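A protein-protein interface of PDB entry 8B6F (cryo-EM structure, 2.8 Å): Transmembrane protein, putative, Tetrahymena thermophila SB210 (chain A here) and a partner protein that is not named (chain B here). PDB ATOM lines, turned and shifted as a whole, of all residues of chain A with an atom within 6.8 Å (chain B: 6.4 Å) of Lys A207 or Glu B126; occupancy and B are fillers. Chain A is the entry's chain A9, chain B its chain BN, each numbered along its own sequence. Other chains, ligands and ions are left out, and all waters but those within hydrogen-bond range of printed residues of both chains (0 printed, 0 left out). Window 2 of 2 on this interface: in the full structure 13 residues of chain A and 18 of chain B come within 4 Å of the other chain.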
ATOM      1  N   SER A 201     -16.370   6.305 -12.446  1.00  0.00           N
ATOM      2  CA  SER A 201     -17.517   5.721 -11.770  1.00  0.00           C
ATOM      3  C   SER A 201     -18.045   6.673 -10.704  1.00  0.00           C
ATOM      4  O   SER A 201     -17.309   7.494 -10.151  1.00  0.00           O
ATOM      5  CB  SER A 201     -17.141   4.380 -11.141  1.00  0.00           C
ATOM      6  OG  SER A 201     -16.062   4.525 -10.234  1.00  0.00           O
ATOM      7  N   GLU A 202     -19.342   6.553 -10.417  1.00  0.00           N
ATOM      8  CA  GLU A 202     -19.953   7.394  -9.394  1.00  0.00           C
ATOM      9  C   GLU A 202     -19.256   7.233  -8.051  1.00  0.00           C
ATOM     10  O   GLU A 202     -19.137   8.202  -7.293  1.00  0.00           O
ATOM     11  CB  GLU A 202     -21.440   7.062  -9.265  1.00  0.00           C
ATOM     12  CG  GLU A 202     -22.209   8.025  -8.380  1.00  0.00           C
ATOM     13  CD  GLU A 202     -23.705   7.783  -8.425  1.00  0.00           C
ATOM     14  OE1 GLU A 202     -24.127   6.792  -9.055  1.00  0.00           O
ATOM     15  OE2 GLU A 202     -24.457   8.586  -7.834  1.00  0.00           O
ATOM     16  N   GLU A 203     -18.782   6.026  -7.743  1.00  0.00           N
ATOM     17  CA  GLU A 203     -18.041   5.818  -6.504  1.00  0.00           C
ATOM     18  C   GLU A 203     -16.762   6.645  -6.485  1.00  0.00           C
ATOM     19  O   GLU A 203     -16.441   7.282  -5.475  1.00  0.00           O
ATOM     20  CB  GLU A 203     -17.719   4.336  -6.327  1.00  0.00           C
ATOM     21  CG  GLU A 203     -18.937   3.462  -6.073  1.00  0.00           C
ATOM     22  CD  GLU A 203     -18.563   2.017  -5.794  1.00  0.00           C
ATOM     23  OE1 GLU A 203     -17.357   1.736  -5.634  1.00  0.00           O
ATOM     24  OE2 GLU A 203     -19.472   1.163  -5.736  1.00  0.00           O
ATOM     25  N   GLU A 204     -16.018   6.651  -7.592  1.00  0.00           N
ATOM     26  CA  GLU A 204     -14.801   7.454  -7.654  1.00  0.00           C
ATOM     27  C   GLU A 204     -15.112   8.939  -7.527  1.00  0.00           C
ATOM     28  O   GLU A 204     -14.389   9.676  -6.845  1.00  0.00           O
ATOM     29  CB  GLU A 204     -14.056   7.176  -8.959  1.00  0.00           C
ATOM     30  CG  GLU A 204     -13.439   5.791  -9.031  1.00  0.00           C
ATOM     31  CD  GLU A 204     -12.809   5.507 -10.380  1.00  0.00           C
ATOM     32  OE1 GLU A 204     -13.212   6.149 -11.372  1.00  0.00           O
ATOM     33  OE2 GLU A 204     -11.904   4.650 -10.446  1.00  0.00           O
ATOM     34  N   ARG A 205     -16.178   9.402  -8.181  1.00  0.00           N
ATOM     35  CA  ARG A 205     -16.549  10.809  -8.074  1.00  0.00           C
ATOM     36  C   ARG A 205     -16.913  11.170  -6.639  1.00  0.00           C
ATOM     37  O   ARG A 205     -16.535  12.237  -6.145  1.00  0.00           O
ATOM     38  CB  ARG A 205     -17.712  11.119  -9.016  1.00  0.00           C
ATOM     39  CG  ARG A 205     -17.464  10.721 -10.461  1.00  0.00           C
ATOM     40  CD  ARG A 205     -18.263  11.590 -11.416  1.00  0.00           C
ATOM     41  NE  ARG A 205     -17.659  12.908 -11.578  1.00  0.00           N
ATOM     42  CZ  ARG A 205     -16.797  13.233 -12.533  1.00  0.00           C
ATOM     43  NH1 ARG A 205     -16.426  12.365 -13.459  1.00  0.00           N
ATOM     44  NH2 ARG A 205     -16.291  14.461 -12.558  1.00  0.00           N
ATOM     45  N   LYS A 206     -17.654  10.294  -5.955  1.00  0.00           N
ATOM     46  CA  LYS A 206     -18.016  10.561  -4.567  1.00  0.00           C
ATOM     47  C   LYS A 206     -16.786  10.577  -3.670  1.00  0.00           C
ATOM     48  O   LYS A 206     -16.690  11.403  -2.754  1.00  0.00           O
ATOM     49  CB  LYS A 206     -19.023   9.525  -4.069  1.00  0.00           C
ATOM     50  CG  LYS A 206     -20.419   9.691  -4.650  1.00  0.00           C
ATOM     51  CD  LYS A 206     -21.442   8.845  -3.902  1.00  0.00           C
ATOM     52  CE  LYS A 206     -21.116   7.361  -3.983  1.00  0.00           C
ATOM     53  NZ  LYS A 206     -22.156   6.524  -3.319  1.00  0.00           N
ATOM     54  N   LYS A 207     -15.835   9.674  -3.914  1.00  0.00           N
ATOM     55  CA  LYS A 207     -14.606   9.676  -3.129  1.00  0.00           C
ATOM     56  C   LYS A 207     -13.829  10.970  -3.334  1.00  0.00           C
ATOM     57  O   LYS A 207     -13.326  11.558  -2.371  1.00  0.00           O
ATOM     58  CB  LYS A 207     -13.751   8.466  -3.503  1.00  0.00           C
ATOM     59  CG  LYS A 207     -12.469   8.332  -2.695  1.00  0.00           C
ATOM     60  CD  LYS A 207     -11.679   7.109  -3.131  1.00  0.00           C
ATOM     61  CE  LYS A 207     -10.368   6.993  -2.374  1.00  0.00           C
ATOM     62  NZ  LYS A 207     -10.573   6.819  -0.912  1.00  0.00           N
ATOM     63  N   GLN A 208     -13.712  11.424  -4.582  1.00  0.00           N
ATOM     64  CA  GLN A 208     -13.019  12.681  -4.841  1.00  0.00           C
ATOM     65  C   GLN A 208     -13.741  13.853  -4.189  1.00  0.00           C
ATOM     66  O   GLN A 208     -13.102  14.767  -3.655  1.00  0.00           O
ATOM     67  CB  GLN A 208     -12.883  12.910  -6.346  1.00  0.00           C
ATOM     68  CG  GLN A 208     -12.111  14.168  -6.708  1.00  0.00           C
ATOM     69  CD  GLN A 208     -10.735  14.213  -6.075  1.00  0.00           C
ATOM     70  OE1 GLN A 208     -10.121  13.178  -5.824  1.00  0.00           O
ATOM     71  NE2 GLN A 208     -10.249  15.417  -5.802  1.00  0.00           N
ATOM     72  N   GLU A 209     -15.075  13.839  -4.213  1.00  0.00           N
ATOM     73  CA  GLU A 209     -15.834  14.906  -3.570  1.00  0.00           C
ATOM     74  C   GLU A 209     -15.674  14.876  -2.058  1.00  0.00           C
ATOM     75  O   GLU A 209     -15.656  15.935  -1.420  1.00  0.00           O
ATOM     76  CB  GLU A 209     -17.309  14.812  -3.959  1.00  0.00           C
ATOM     77  CG  GLU A 209     -17.585  15.246  -5.390  1.00  0.00           C
ATOM     78  CD  GLU A 209     -19.062  15.274  -5.726  1.00  0.00           C
ATOM     79  OE1 GLU A 209     -19.878  14.900  -4.859  1.00  0.00           O
ATOM     80  OE2 GLU A 209     -19.408  15.672  -6.857  1.00  0.00           O
ATOM     81  N   TYR A 210     -15.561  13.687  -1.462  1.00  0.00           N
ATOM     82  CA  TYR A 210     -15.273  13.618  -0.034  1.00  0.00           C
ATOM     83  C   TYR A 210     -13.911  14.222   0.276  1.00  0.00           C
ATOM     84  O   TYR A 210     -13.759  14.955   1.258  1.00  0.00           O
ATOM     85  CB  TYR A 210     -15.340  12.170   0.451  1.00  0.00           C
ATOM     86  CG  TYR A 210     -16.712  11.538   0.348  1.00  0.00           C
ATOM     87  CD1 TYR A 210     -17.862  12.318   0.303  1.00  0.00           C
ATOM     88  CD2 TYR A 210     -16.856  10.160   0.301  1.00  0.00           C
ATOM     89  CE1 TYR A 210     -19.112  11.743   0.211  1.00  0.00           C
ATOM     90  CE2 TYR A 210     -18.104   9.576   0.209  1.00  0.00           C
ATOM     91  CZ  TYR A 210     -19.226  10.373   0.164  1.00  0.00           C
ATOM     92  OH  TYR A 210     -20.471   9.797   0.073  1.00  0.00           O
ATOM     93  N   LYS A 211     -12.904  13.925  -0.549  1.00  0.00           N
ATOM     94  CA  LYS A 211     -11.599  14.549  -0.364  1.00  0.00           C
ATOM     95  C   LYS A 211     -11.693  16.061  -0.511  1.00  0.00           C
ATOM     96  O   LYS A 211     -11.068  16.808   0.250  1.00  0.00           O
ATOM     97  CB  LYS A 211     -10.596  13.980  -1.365  1.00  0.00           C
ATOM     98  CG  LYS A 211     -10.109  12.584  -1.029  1.00  0.00           C
ATOM     99  CD  LYS A 211      -8.952  12.187  -1.925  1.00  0.00           C
ATOM    100  CE  LYS A 211      -8.359  10.854  -1.510  1.00  0.00           C
ATOM    101  NZ  LYS A 211      -7.154  10.523  -2.321  1.00  0.00           N
ATOM    102  N   ASP A 212     -12.466  16.530  -1.491  1.00  0.00           N
ATOM    103  CA  ASP A 212     -12.631  17.966  -1.683  1.00  0.00           C
ATOM    104  C   ASP A 212     -13.297  18.606  -0.475  1.00  0.00           C
ATOM    105  O   ASP A 212     -12.926  19.710  -0.063  1.00  0.00           O
ATOM    106  CB  ASP A 212     -13.444  18.242  -2.947  1.00  0.00           C
ATOM    107  CG  ASP A 212     -12.680  17.920  -4.211  1.00  0.00           C
ATOM    108  OD1 ASP A 212     -11.492  17.551  -4.111  1.00  0.00           O
ATOM    109  OD2 ASP A 212     -13.265  18.040  -5.308  1.00  0.00           O
ATOM    110  N   HIS B 115     -19.054   3.061   7.570  1.00  0.00           N
ATOM    111  CA  HIS B 115     -17.715   2.641   7.173  1.00  0.00           C
ATOM    112  C   HIS B 115     -16.999   1.943   8.321  1.00  0.00           C
ATOM    113  O   HIS B 115     -16.322   0.929   8.117  1.00  0.00           O
ATOM    114  CB  HIS B 115     -16.912   3.851   6.692  1.00  0.00           C
ATOM    115  CG  HIS B 115     -15.555   3.506   6.165  1.00  0.00           C
ATOM    116  ND1 HIS B 115     -14.454   3.355   6.980  1.00  0.00           N
ATOM    117  CD2 HIS B 115     -15.120   3.289   4.901  1.00  0.00           C
ATOM    118  CE1 HIS B 115     -13.400   3.056   6.242  1.00  0.00           C
ATOM    119  NE2 HIS B 115     -13.777   3.010   4.976  1.00  0.00           N
ATOM    120  N   PHE B 124     -14.288  -3.765   3.390  1.00  0.00           N
ATOM    121  CA  PHE B 124     -13.575  -2.495   3.471  1.00  0.00           C
ATOM    122  C   PHE B 124     -14.050  -1.608   2.331  1.00  0.00           C
ATOM    123  O   PHE B 124     -13.856  -1.948   1.159  1.00  0.00           O
ATOM    124  CB  PHE B 124     -12.060  -2.701   3.400  1.00  0.00           C
ATOM    125  CG  PHE B 124     -11.282  -1.420   3.311  1.00  0.00           C
ATOM    126  CD1 PHE B 124     -10.951  -0.714   4.455  1.00  0.00           C
ATOM    127  CD2 PHE B 124     -10.881  -0.924   2.080  1.00  0.00           C
ATOM    128  CE1 PHE B 124     -10.234   0.464   4.375  1.00  0.00           C
ATOM    129  CE2 PHE B 124     -10.165   0.254   1.993  1.00  0.00           C
ATOM    130  CZ  PHE B 124      -9.843   0.949   3.142  1.00  0.00           C
ATOM    131  N   VAL B 125     -14.661  -0.478   2.670  1.00  0.00           N
ATOM    132  CA  VAL B 125     -15.223   0.441   1.687  1.00  0.00           C
ATOM    133  C   VAL B 125     -14.236   1.581   1.480  1.00  0.00           C
ATOM    134  O   VAL B 125     -13.918   2.318   2.421  1.00  0.00           O
ATOM    135  CB  VAL B 125     -16.594   0.971   2.133  1.00  0.00           C
ATOM    136  CG1 VAL B 125     -17.219   1.823   1.038  1.00  0.00           C
ATOM    137  CG2 VAL B 125     -17.513  -0.178   2.505  1.00  0.00           C
ATOM    138  N   GLU B 126     -13.757   1.733   0.247  1.00  0.00           N
ATOM    139  CA  GLU B 126     -12.808   2.787  -0.080  1.00  0.00           C
ATOM    140  C   GLU B 126     -13.481   4.097  -0.460  1.00  0.00           C
ATOM    141  O   GLU B 126     -12.838   5.150  -0.391  1.00  0.00           O
ATOM    142  CB  GLU B 126     -11.904   2.336  -1.232  1.00  0.00           C
ATOM    143  CG  GLU B 126     -10.780   3.307  -1.557  1.00  0.00           C
ATOM    144  CD  GLU B 126      -9.886   2.805  -2.673  1.00  0.00           C
ATOM    145  OE1 GLU B 126     -10.251   1.802  -3.320  1.00  0.00           O
ATOM    146  OE2 GLU B 126      -8.818   3.412  -2.902  1.00  0.00           O
ATOM    147  N   THR B 127     -14.755   4.061  -0.856  1.00  0.00           N
ATOM    148  CA  THR B 127     -15.424   5.278  -1.302  1.00  0.00           C
ATOM    149  C   THR B 127     -15.522   6.302  -0.180  1.00  0.00           C
ATOM    150  O   THR B 127     -15.285   7.496  -0.397  1.00  0.00           O
ATOM    151  CB  THR B 127     -16.816   4.945  -1.838  1.00  0.00           C
ATOM    152  OG1 THR B 127     -17.631   4.435  -0.777  1.00  0.00           O
ATOM    153  CG2 THR B 127     -16.724   3.908  -2.941  1.00  0.00           C
ATOM    154  N   THR B 128     -15.869   5.857   1.026  1.00  0.00           N
ATOM    155  CA  THR B 128     -16.075   6.744   2.162  1.00  0.00           C
ATOM    156  C   THR B 128     -14.868   6.807   3.086  1.00  0.00           C
ATOM    157  O   THR B 128     -14.965   7.377   4.176  1.00  0.00           O
ATOM    158  CB  THR B 128     -17.308   6.306   2.955  1.00  0.00           C
ATOM    159  OG1 THR B 128     -17.166   4.935   3.350  1.00  0.00           O
ATOM    160  CG2 THR B 128     -18.567   6.463   2.119  1.00  0.00           C
ATOM    161  N   SER B 129     -13.736   6.233   2.682  1.00  0.00           N
ATOM    162  CA  SER B 129     -12.559   6.248   3.545  1.00  0.00           C
ATOM    163  C   SER B 129     -12.128   7.655   3.941  1.00  0.00           C
ATOM    164  O   SER B 129     -11.752   7.843   5.112  1.00  0.00           O
ATOM    165  CB  SER B 129     -11.407   5.493   2.867  1.00  0.00           C
ATOM    166  OG  SER B 129     -11.137   5.992   1.571  1.00  0.00           O
ATOM    167  N   PRO B 130     -12.145   8.662   3.065  1.00  0.00           N
ATOM    168  CA  PRO B 130     -11.663   9.991   3.480  1.00  0.00           C
ATOM    169  C   PRO B 130     -12.453  10.597   4.627  1.00  0.00           C
ATOM    170  O   PRO B 130     -11.923  11.465   5.329  1.00  0.00           O
ATOM    171  CB  PRO B 130     -11.798  10.832   2.201  1.00  0.00           C
ATOM    172  CG  PRO B 130     -11.906   9.852   1.091  1.00  0.00           C
ATOM    173  CD  PRO B 130     -12.613   8.675   1.668  1.00  0.00           C
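The backbone carbonyl oxygen (O) of Glu B126 lies within hydrogen-bond range of the side-chain hydroxyl (OG) of Ser B129, at 2.7 Å.
OE1 of Glu A203 touches CG2 of Thr B127 (3.5 Å).
CA of Lys A207 touches O of Thr B127, 3.6 Å away.
CD of Pro B130 touches NZ of Lys A207 (3.8 Å).
Tyr A210 touches Thr B127 (CD2 to O, 3.2 Å).
CE2 of Tyr A210 touches CG2 of Thr B128, at 3.7 Å.
Lys A211 touches Pro B130 (CG to CG, 3.9 Å).
Of chain A, only Lys A207 comes within 4 Å of Glu B126.
Of the printed residues of chain B, Tyr A210 touches Thr B127 (3.2 Å) and Thr B128 (3.7 Å).
Of the printed residues of chain A, Thr B127 touches Glu A203, Lys A207 and Tyr A210.
Printed residues of chain B within 4 Å of Lys A211: Pro B130 (3.9 Å).
Of the printed residues of chain B, Glu A203 touches Thr B127 (3.5 Å).
Gln A208 touches none of the printed residues of chain B.
Glu A202 touches none of the printed residues of chain B.
The nearest residue of chain B that does not touch Lys A207 is Thr B128 (5.6 Å).
Printed residues of chain A that touch a printed residue of chain B: Glu A203, Lys A207, Tyr A210 and Lys A211.
Along chain A the printed residues that touch a printed residue of chain B span positions 203 to 211.
Among the printed residues, 8 pairs touch across the chains.
O of Glu B126 sits at hydrogen-bond distance from NZ of Lys A207.
NZ of Lys A207 sits at hydrogen-bond distance from OG of Ser B129, 2.7 Å away.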
